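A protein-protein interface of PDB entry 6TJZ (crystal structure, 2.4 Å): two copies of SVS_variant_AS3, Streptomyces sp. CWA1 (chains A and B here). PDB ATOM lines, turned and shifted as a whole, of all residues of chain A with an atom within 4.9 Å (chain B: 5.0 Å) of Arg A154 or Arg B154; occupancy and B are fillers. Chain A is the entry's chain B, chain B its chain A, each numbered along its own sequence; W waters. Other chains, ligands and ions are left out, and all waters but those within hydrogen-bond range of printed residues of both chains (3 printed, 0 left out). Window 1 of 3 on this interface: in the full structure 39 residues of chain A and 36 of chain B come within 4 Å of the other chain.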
ATOM      1  N   GLN A 111     -12.186   6.232 -18.242  1.00  0.00           N
ATOM      2  CA  GLN A 111     -12.118   4.947 -17.492  1.00  0.00           C
ATOM      3  C   GLN A 111     -11.927   3.794 -18.490  1.00  0.00           C
ATOM      4  O   GLN A 111     -11.120   2.896 -18.212  1.00  0.00           O
ATOM      5  CB  GLN A 111     -13.385   4.768 -16.647  1.00  0.00           C
ATOM      6  CG  GLN A 111     -13.373   3.523 -15.779  1.00  0.00           C
ATOM      7  CD  GLN A 111     -12.325   3.566 -14.697  1.00  0.00           C
ATOM      8  OE1 GLN A 111     -11.880   4.636 -14.266  1.00  0.00           O
ATOM      9  NE2 GLN A 111     -11.946   2.390 -14.222  1.00  0.00           N
ATOM     10  N   GLU A 115      -8.614   1.026 -18.799  1.00  0.00           N
ATOM     11  CA  GLU A 115      -8.842  -0.444 -18.802  1.00  0.00           C
ATOM     12  C   GLU A 115      -8.489  -1.083 -20.156  1.00  0.00           C
ATOM     13  O   GLU A 115      -8.369  -2.304 -20.199  1.00  0.00           O
ATOM     14  CB  GLU A 115     -10.318  -0.718 -18.527  1.00  0.00           C
ATOM     15  CG  GLU A 115     -10.763  -0.291 -17.143  1.00  0.00           C
ATOM     16  CD  GLU A 115     -12.091  -0.847 -16.648  1.00  0.00           C
ATOM     17  OE1 GLU A 115     -12.838  -0.069 -16.006  1.00  0.00           O
ATOM     18  OE2 GLU A 115     -12.365  -2.058 -16.860  1.00  0.00           O
ATOM     19  N   VAL A 150      -7.871   0.399 -10.940  1.00  0.00           N
ATOM     20  CA  VAL A 150      -8.941   0.591 -11.956  1.00  0.00           C
ATOM     21  C   VAL A 150     -10.270   0.811 -11.234  1.00  0.00           C
ATOM     22  O   VAL A 150     -10.916   1.818 -11.491  1.00  0.00           O
ATOM     23  CB  VAL A 150      -8.992  -0.594 -12.941  1.00  0.00           C
ATOM     24  CG1 VAL A 150     -10.334  -0.707 -13.621  1.00  0.00           C
ATOM     25  CG2 VAL A 150      -7.904  -0.477 -13.984  1.00  0.00           C
ATOM     26  N   HIS A 151     -10.650  -0.093 -10.343  1.00  0.00           N
ATOM     27  CA  HIS A 151     -11.933  -0.038  -9.605  1.00  0.00           C
ATOM     28  C   HIS A 151     -11.991   1.217  -8.726  1.00  0.00           C
ATOM     29  O   HIS A 151     -13.073   1.844  -8.632  1.00  0.00           O
ATOM     30  CB  HIS A 151     -12.081  -1.314  -8.785  1.00  0.00           C
ATOM     31  CG  HIS A 151     -12.339  -2.494  -9.645  1.00  0.00           C
ATOM     32  ND1 HIS A 151     -13.188  -2.413 -10.736  1.00  0.00           N
ATOM     33  CD2 HIS A 151     -11.912  -3.777  -9.574  1.00  0.00           C
ATOM     34  CE1 HIS A 151     -13.275  -3.602 -11.308  1.00  0.00           C
ATOM     35  NE2 HIS A 151     -12.508  -4.453 -10.613  1.00  0.00           N
ATOM     36  N   ALA A 152     -10.887   1.544  -8.057  1.00  0.00           N
ATOM     37  CA  ALA A 152     -10.773   2.778  -7.257  1.00  0.00           C
ATOM     38  C   ALA A 152     -10.972   4.000  -8.160  1.00  0.00           C
ATOM     39  O   ALA A 152     -11.712   4.909  -7.740  1.00  0.00           O
ATOM     40  CB  ALA A 152      -9.450   2.825  -6.549  1.00  0.00           C
ATOM     41  N   HIS A 153     -10.360   4.016  -9.353  1.00  0.00           N
ATOM     42  CA  HIS A 153     -10.467   5.134 -10.322  1.00  0.00           C
ATOM     43  C   HIS A 153     -11.931   5.332 -10.742  1.00  0.00           C
ATOM     44  O   HIS A 153     -12.386   6.476 -10.777  1.00  0.00           O
ATOM     45  CB  HIS A 153      -9.545   4.900 -11.510  1.00  0.00           C
ATOM     46  CG  HIS A 153      -9.233   6.134 -12.284  1.00  0.00           C
ATOM     47  ND1 HIS A 153     -10.019   6.550 -13.356  1.00  0.00           N
ATOM     48  CD2 HIS A 153      -8.201   7.003 -12.197  1.00  0.00           C
ATOM     49  CE1 HIS A 153      -9.472   7.628 -13.895  1.00  0.00           C
ATOM     50  NE2 HIS A 153      -8.364   7.939 -13.193  1.00  0.00           N
ATOM     51  N   ARG A 154     -12.664   4.257 -11.024  1.00  0.00           N
ATOM     52  CA  ARG A 154     -14.102   4.369 -11.377  1.00  0.00           C
ATOM     53  C   ARG A 154     -14.851   4.898 -10.160  1.00  0.00           C
ATOM     54  O   ARG A 154     -15.694   5.761 -10.367  1.00  0.00           O
ATOM     55  CB  ARG A 154     -14.716   3.058 -11.874  1.00  0.00           C
ATOM     56  CG  ARG A 154     -16.157   3.229 -12.320  1.00  0.00           C
ATOM     57  CD  ARG A 154     -16.846   1.970 -12.785  1.00  0.00           C
ATOM     58  NE  ARG A 154     -16.450   1.735 -14.158  1.00  0.00           N
ATOM     59  CZ  ARG A 154     -15.686   0.745 -14.576  1.00  0.00           C
ATOM     60  NH1 ARG A 154     -15.233  -0.163 -13.728  1.00  0.00           N
ATOM     61  NH2 ARG A 154     -15.394   0.665 -15.860  1.00  0.00           N
ATOM     62  N   ALA A 155     -14.525   4.457  -8.939  1.00  0.00           N
ATOM     63  CA  ALA A 155     -15.233   4.919  -7.713  1.00  0.00           C
ATOM     64  C   ALA A 155     -15.085   6.448  -7.597  1.00  0.00           C
ATOM     65  O   ALA A 155     -16.115   7.177  -7.438  1.00  0.00           O
ATOM     66  CB  ALA A 155     -14.724   4.179  -6.511  1.00  0.00           C
ATOM     67  N   TYR A 156     -13.865   6.943  -7.787  1.00  0.00           N
ATOM     68  CA  TYR A 156     -13.558   8.388  -7.839  1.00  0.00           C
ATOM     69  C   TYR A 156     -14.381   9.077  -8.942  1.00  0.00           C
ATOM     70  O   TYR A 156     -14.968  10.125  -8.668  1.00  0.00           O
ATOM     71  CB  TYR A 156     -12.057   8.574  -8.012  1.00  0.00           C
ATOM     72  CG  TYR A 156     -11.614   9.891  -8.577  1.00  0.00           C
ATOM     73  CD1 TYR A 156     -11.792  11.071  -7.869  1.00  0.00           C
ATOM     74  CD2 TYR A 156     -10.952   9.949  -9.793  1.00  0.00           C
ATOM     75  CE1 TYR A 156     -11.342  12.284  -8.373  1.00  0.00           C
ATOM     76  CE2 TYR A 156     -10.486  11.152 -10.307  1.00  0.00           C
ATOM     77  CZ  TYR A 156     -10.669  12.316  -9.584  1.00  0.00           C
ATOM     78  OH  TYR A 156     -10.234  13.500 -10.099  1.00  0.00           O
ATOM     79  N   LEU A 157     -14.419   8.543 -10.153  1.00  0.00           N
ATOM     80  CA  LEU A 157     -15.123   9.212 -11.273  1.00  0.00           C
ATOM     81  C   LEU A 157     -16.618   9.312 -10.930  1.00  0.00           C
ATOM     82  O   LEU A 157     -17.149  10.410 -11.119  1.00  0.00           O
ATOM     83  CB  LEU A 157     -14.833   8.487 -12.590  1.00  0.00           C
ATOM     84  CG  LEU A 157     -13.417   8.714 -13.125  1.00  0.00           C
ATOM     85  CD1 LEU A 157     -13.136   7.845 -14.349  1.00  0.00           C
ATOM     86  CD2 LEU A 157     -13.179  10.184 -13.464  1.00  0.00           C
ATOM     87  N   SER A 158     -17.221   8.283 -10.308  1.00  0.00           N
ATOM     88  CA  SER A 158     -18.611   8.291  -9.767  1.00  0.00           C
ATOM     89  C   SER A 158     -18.831   9.395  -8.726  1.00  0.00           C
ATOM     90  O   SER A 158     -19.941   9.999  -8.705  1.00  0.00           O
ATOM     91  CB  SER A 158     -18.975   6.975  -9.181  1.00  0.00           C
ATOM     92  OG  SER A 158     -18.871   5.958 -10.175  1.00  0.00           O
ATOM     93  N   LEU A 184     -15.489   9.438  -2.320  1.00  0.00           N
ATOM     94  CA  LEU A 184     -15.111   9.121  -3.712  1.00  0.00           C
ATOM     95  C   LEU A 184     -14.569  10.356  -4.418  1.00  0.00           C
ATOM     96  O   LEU A 184     -13.638  10.185  -5.161  1.00  0.00           O
ATOM     97  CB  LEU A 184     -16.340   8.593  -4.441  1.00  0.00           C
ATOM     98  CG  LEU A 184     -17.029   7.406  -3.781  1.00  0.00           C
ATOM     99  CD1 LEU A 184     -18.281   7.059  -4.553  1.00  0.00           C
ATOM    100  CD2 LEU A 184     -16.080   6.199  -3.685  1.00  0.00           C
ATOM    101  N   GLN B 111     -25.205   2.502  -4.749  1.00  0.00           N
ATOM    102  CA  GLN B 111     -23.889   1.822  -4.661  1.00  0.00           C
ATOM    103  C   GLN B 111     -23.409   1.814  -3.190  1.00  0.00           C
ATOM    104  O   GLN B 111     -22.873   0.773  -2.726  1.00  0.00           O
ATOM    105  CB  GLN B 111     -22.911   2.485  -5.627  1.00  0.00           C
ATOM    106  CG  GLN B 111     -21.585   1.747  -5.740  1.00  0.00           C
ATOM    107  CD  GLN B 111     -21.647   0.310  -6.232  1.00  0.00           C
ATOM    108  OE1 GLN B 111     -22.551  -0.099  -6.962  1.00  0.00           O
ATOM    109  NE2 GLN B 111     -20.648  -0.482  -5.840  1.00  0.00           N
ATOM    110  N   GLU B 115     -22.309  -1.294  -0.391  1.00  0.00           N
ATOM    111  CA  GLU B 115     -20.962  -1.426   0.247  1.00  0.00           C
ATOM    112  C   GLU B 115     -21.061  -1.236   1.764  1.00  0.00           C
ATOM    113  O   GLU B 115     -20.122  -1.637   2.457  1.00  0.00           O
ATOM    114  CB  GLU B 115     -19.954  -0.398  -0.288  1.00  0.00           C
ATOM    115  CG  GLU B 115     -19.958  -0.296  -1.798  1.00  0.00           C
ATOM    116  CD  GLU B 115     -18.743   0.293  -2.497  1.00  0.00           C
ATOM    117  OE1 GLU B 115     -17.703   0.453  -1.850  1.00  0.00           O
ATOM    118  OE2 GLU B 115     -18.851   0.568  -3.729  1.00  0.00           O
ATOM    119  N   VAL B 150     -19.320  -5.979  -6.103  1.00  0.00           N
ATOM    120  CA  VAL B 150     -19.541  -4.553  -5.758  1.00  0.00           C
ATOM    121  C   VAL B 150     -18.853  -3.704  -6.829  1.00  0.00           C
ATOM    122  O   VAL B 150     -19.450  -2.744  -7.309  1.00  0.00           O
ATOM    123  CB  VAL B 150     -19.009  -4.235  -4.349  1.00  0.00           C
ATOM    124  CG1 VAL B 150     -18.816  -2.754  -4.161  1.00  0.00           C
ATOM    125  CG2 VAL B 150     -19.890  -4.803  -3.247  1.00  0.00           C
ATOM    126  N   HIS B 151     -17.619  -4.019  -7.182  1.00  0.00           N
ATOM    127  CA  HIS B 151     -16.925  -3.282  -8.269  1.00  0.00           C
ATOM    128  C   HIS B 151     -17.698  -3.414  -9.595  1.00  0.00           C
ATOM    129  O   HIS B 151     -17.814  -2.405 -10.322  1.00  0.00           O
ATOM    130  CB  HIS B 151     -15.472  -3.742  -8.397  1.00  0.00           C
ATOM    131  CG  HIS B 151     -14.633  -3.321  -7.239  1.00  0.00           C
ATOM    132  ND1 HIS B 151     -14.700  -2.040  -6.709  1.00  0.00           N
ATOM    133  CD2 HIS B 151     -13.680  -3.979  -6.543  1.00  0.00           C
ATOM    134  CE1 HIS B 151     -13.826  -1.932  -5.731  1.00  0.00           C
ATOM    135  NE2 HIS B 151     -13.191  -3.105  -5.613  1.00  0.00           N
ATOM    136  N   ALA B 152     -18.172  -4.611  -9.928  1.00  0.00           N
ATOM    137  CA  ALA B 152     -18.888  -4.882 -11.195  1.00  0.00           C
ATOM    138  C   ALA B 152     -20.181  -4.068 -11.174  1.00  0.00           C
ATOM    139  O   ALA B 152     -20.581  -3.524 -12.211  1.00  0.00           O
ATOM    140  CB  ALA B 152     -19.166  -6.359 -11.349  1.00  0.00           C
ATOM    141  N   HIS B 153     -20.768  -3.942  -9.989  1.00  0.00           N
ATOM    142  CA  HIS B 153     -22.026  -3.196  -9.785  1.00  0.00           C
ATOM    143  C   HIS B 153     -21.813  -1.705 -10.105  1.00  0.00           C
ATOM    144  O   HIS B 153     -22.622  -1.135 -10.823  1.00  0.00           O
ATOM    145  CB  HIS B 153     -22.571  -3.496  -8.390  1.00  0.00           C
ATOM    146  CG  HIS B 153     -24.010  -3.158  -8.281  1.00  0.00           C
ATOM    147  ND1 HIS B 153     -24.436  -1.897  -7.919  1.00  0.00           N
ATOM    148  CD2 HIS B 153     -25.110  -3.891  -8.525  1.00  0.00           C
ATOM    149  CE1 HIS B 153     -25.755  -1.887  -7.915  1.00  0.00           C
ATOM    150  NE2 HIS B 153     -26.195  -3.092  -8.301  1.00  0.00           N
ATOM    151  N   ARG B 154     -20.757  -1.070  -9.626  1.00  0.00           N
ATOM    152  CA  ARG B 154     -20.537   0.374  -9.903  1.00  0.00           C
ATOM    153  C   ARG B 154     -20.264   0.558 -11.412  1.00  0.00           C
ATOM    154  O   ARG B 154     -20.694   1.571 -12.001  1.00  0.00           O
ATOM    155  CB  ARG B 154     -19.400   0.903  -9.025  1.00  0.00           C
ATOM    156  CG  ARG B 154     -19.198   2.412  -9.135  1.00  0.00           C
ATOM    157  CD  ARG B 154     -17.992   2.946  -8.378  1.00  0.00           C
ATOM    158  NE  ARG B 154     -17.953   2.714  -6.934  1.00  0.00           N
ATOM    159  CZ  ARG B 154     -18.661   3.409  -6.043  1.00  0.00           C
ATOM    160  NH1 ARG B 154     -19.526   4.361  -6.412  1.00  0.00           N
ATOM    161  NH2 ARG B 154     -18.509   3.125  -4.760  1.00  0.00           N
ATOM    162  N   ALA B 155     -19.578  -0.396 -12.034  1.00  0.00           N
ATOM    163  CA  ALA B 155     -19.283  -0.396 -13.482  1.00  0.00           C
ATOM    164  C   ALA B 155     -20.605  -0.342 -14.257  1.00  0.00           C
ATOM    165  O   ALA B 155     -20.754   0.544 -15.124  1.00  0.00           O
ATOM    166  CB  ALA B 155     -18.466  -1.621 -13.809  1.00  0.00           C
ATOM    167  N   TYR B 156     -21.548  -1.232 -13.923  1.00  0.00           N
ATOM    168  CA  TYR B 156     -22.906  -1.269 -14.513  1.00  0.00           C
ATOM    169  C   TYR B 156     -23.546   0.120 -14.360  1.00  0.00           C
ATOM    170  O   TYR B 156     -24.096   0.676 -15.332  1.00  0.00           O
ATOM    171  CB  TYR B 156     -23.724  -2.368 -13.832  1.00  0.00           C
ATOM    172  CG  TYR B 156     -25.227  -2.171 -13.789  1.00  0.00           C
ATOM    173  CD1 TYR B 156     -25.962  -1.982 -14.947  1.00  0.00           C
ATOM    174  CD2 TYR B 156     -25.931  -2.252 -12.593  1.00  0.00           C
ATOM    175  CE1 TYR B 156     -27.343  -1.889 -14.926  1.00  0.00           C
ATOM    176  CE2 TYR B 156     -27.312  -2.128 -12.552  1.00  0.00           C
ATOM    177  CZ  TYR B 156     -28.021  -1.950 -13.722  1.00  0.00           C
ATOM    178  OH  TYR B 156     -29.379  -1.814 -13.705  1.00  0.00           O
ATOM    179  N   LEU B 157     -23.524   0.670 -13.146  1.00  0.00           N
ATOM    180  CA  LEU B 157     -24.183   1.970 -12.854  1.00  0.00           C
ATOM    181  C   LEU B 157     -23.496   3.080 -13.642  1.00  0.00           C
ATOM    182  O   LEU B 157     -24.235   3.970 -14.137  1.00  0.00           O
ATOM    183  CB  LEU B 157     -24.164   2.254 -11.357  1.00  0.00           C
ATOM    184  CG  LEU B 157     -25.100   1.374 -10.533  1.00  0.00           C
ATOM    185  CD1 LEU B 157     -24.924   1.671  -9.046  1.00  0.00           C
ATOM    186  CD2 LEU B 157     -26.550   1.565 -10.957  1.00  0.00           C
ATOM    187  N   SER B 158     -22.166   3.045 -13.781  1.00  0.00           N
ATOM    188  CA  SER B 158     -21.435   4.063 -14.594  1.00  0.00           C
ATOM    189  C   SER B 158     -21.968   4.026 -16.025  1.00  0.00           C
ATOM    190  O   SER B 158     -22.131   5.089 -16.605  1.00  0.00           O
ATOM    191  CB  SER B 158     -19.946   3.896 -14.587  1.00  0.00           C
ATOM    192  OG  SER B 158     -19.429   4.233 -13.316  1.00  0.00           O
ATOM    193  N   GLY B 159     -22.202   2.831 -16.565  1.00  0.00           N
ATOM    194  CA  GLY B 159     -22.736   2.648 -17.928  1.00  0.00           C
ATOM    195  C   GLY B 159     -24.104   3.295 -18.081  1.00  0.00           C
ATOM    196  O   GLY B 159     -24.340   3.923 -19.132  1.00  0.00           O
ATOM    197  N   LEU B 184     -21.186  -1.952 -20.080  1.00  0.00           N
ATOM    198  CA  LEU B 184     -21.517  -1.664 -18.668  1.00  0.00           C
ATOM    199  C   LEU B 184     -23.037  -1.606 -18.465  1.00  0.00           C
ATOM    200  O   LEU B 184     -23.528  -2.236 -17.501  1.00  0.00           O
ATOM    201  CB  LEU B 184     -20.836  -0.346 -18.288  1.00  0.00           C
ATOM    202  CG  LEU B 184     -19.317  -0.311 -18.445  1.00  0.00           C
ATOM    203  CD1 LEU B 184     -18.754   1.025 -17.991  1.00  0.00           C
ATOM    204  CD2 LEU B 184     -18.647  -1.464 -17.681  1.00  0.00           C
HETATM  205  O   HOH W   1     -15.858  -0.551 -10.821  1.00  0.00           O
HETATM  206  O   HOH W   2     -15.507   0.615  -8.595  1.00  0.00           O
HETATM  207  O   HOH W   3     -20.963   4.647 -10.985  1.00  0.00           O
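Among the printed residues, pairs that only touch across the chains: His A151 with His B151 (3.4 Å), Ala A155 with Arg B154 (3.5 Å), Arg A154 with Ala B155 (3.5 Å), Arg A154 with Ser B158 (3.5 Å), Leu A184 with Arg B154 (3.5 Å), Ser A158 with Arg B154 (3.6 Å), Ser A158 with Ser B158 (3.6 Å), Arg A154 with Arg B154 (3.9 Å) and Arg A154 with Leu B184 (3.995 Å).
Of the printed residues of chain B, Arg A154 touches Arg B154, Ala B155, Ser B158 and Leu B184.
Of the printed residues of chain B, Ser A158 touches Arg B154 and Ser B158.
Of the printed residues of chain A, Ser B158 touches Arg A154 (3.5 Å) and Ser A158 (3.6 Å).
Printed residues of chain A within 4 Å of His B151: His A151.
Of the printed residues of chain A, Leu B184 touches Arg A154 (3.995 Å).
His B153 touches none of the printed residues of chain A.
Gln A111 touches none of the printed residues of chain B.
The nearest printed residue of chain A that does not touch Arg B154 is His A151 (5.0 Å).
Of the 13 printed residues of chain B, 5 touch a printed residue of chain A.
Among the printed residues, no Asp or Glu carboxylate lies within 4 Å of a Lys or Arg side-chain nitrogen of the other chain.
His B151 touches its own counterpart, His A151.
Arg A154 touches Ala B155, and with the chains exchanged Ala A155 touches Arg B154.
Arg A154 touches Ser B158, and with the chains exchanged Ser A158 touches Arg B154.
Arg A154 touches Leu B184, and with the chains exchanged Leu A184 touches Arg B154.
Positions printed for both chains: 111, 115, 150, 151, 152, 153, 154, 155, 156, 157, 158 and 184.
Of the 9 pairs that touch across the chains among the printed residues, 9 have their exchanged pair printed and touching as well.
Water W3 lies within hydrogen-bond range of OG of Ser A158, OG of Ser B158 and O of Arg B154.
Water W2 bridges the backbone carbonyl oxygen of His A151 (2.7 Å) and a ring nitrogen (ND1) of His B151 (3.4 Å).
Water W1 lies within hydrogen-bond range of the backbone carbonyl oxygen of His B151 (2.7 Å), the guanidinium group of Arg A154 (3.0 Å) and a ring nitrogen (ND1) of His A151 (3.3 Å).
The side-chain amide oxygen of Gln B111 is in hydrogen-bond range of the backbone NH of Arg B154 (3.4 Å).
OE2 of Glu B115 lies within salt-bridge range of NH2 of Arg B154, 2.8 Å away.
The backbone carbonyl oxygen (O) of Arg B154 lies within hydrogen-bond range of the side-chain hydroxyl (OG) of Ser B158 (3.2 Å).
The backbone NH (N) of Arg A154 sits at hydrogen-bond distance from the side-chain amide oxygen (OE1) of Gln A111 (3.4 Å).
The guanidinium group (NH2) of Arg A154 is in salt-bridge range of the side-chain carboxylate (OE1) of Glu A115, 2.7 Å away.
The backbone carbonyl oxygen (O) of Arg A154 is in hydrogen-bond range of the side-chain hydroxyl (OG) of Ser A158 (3.2 Å).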
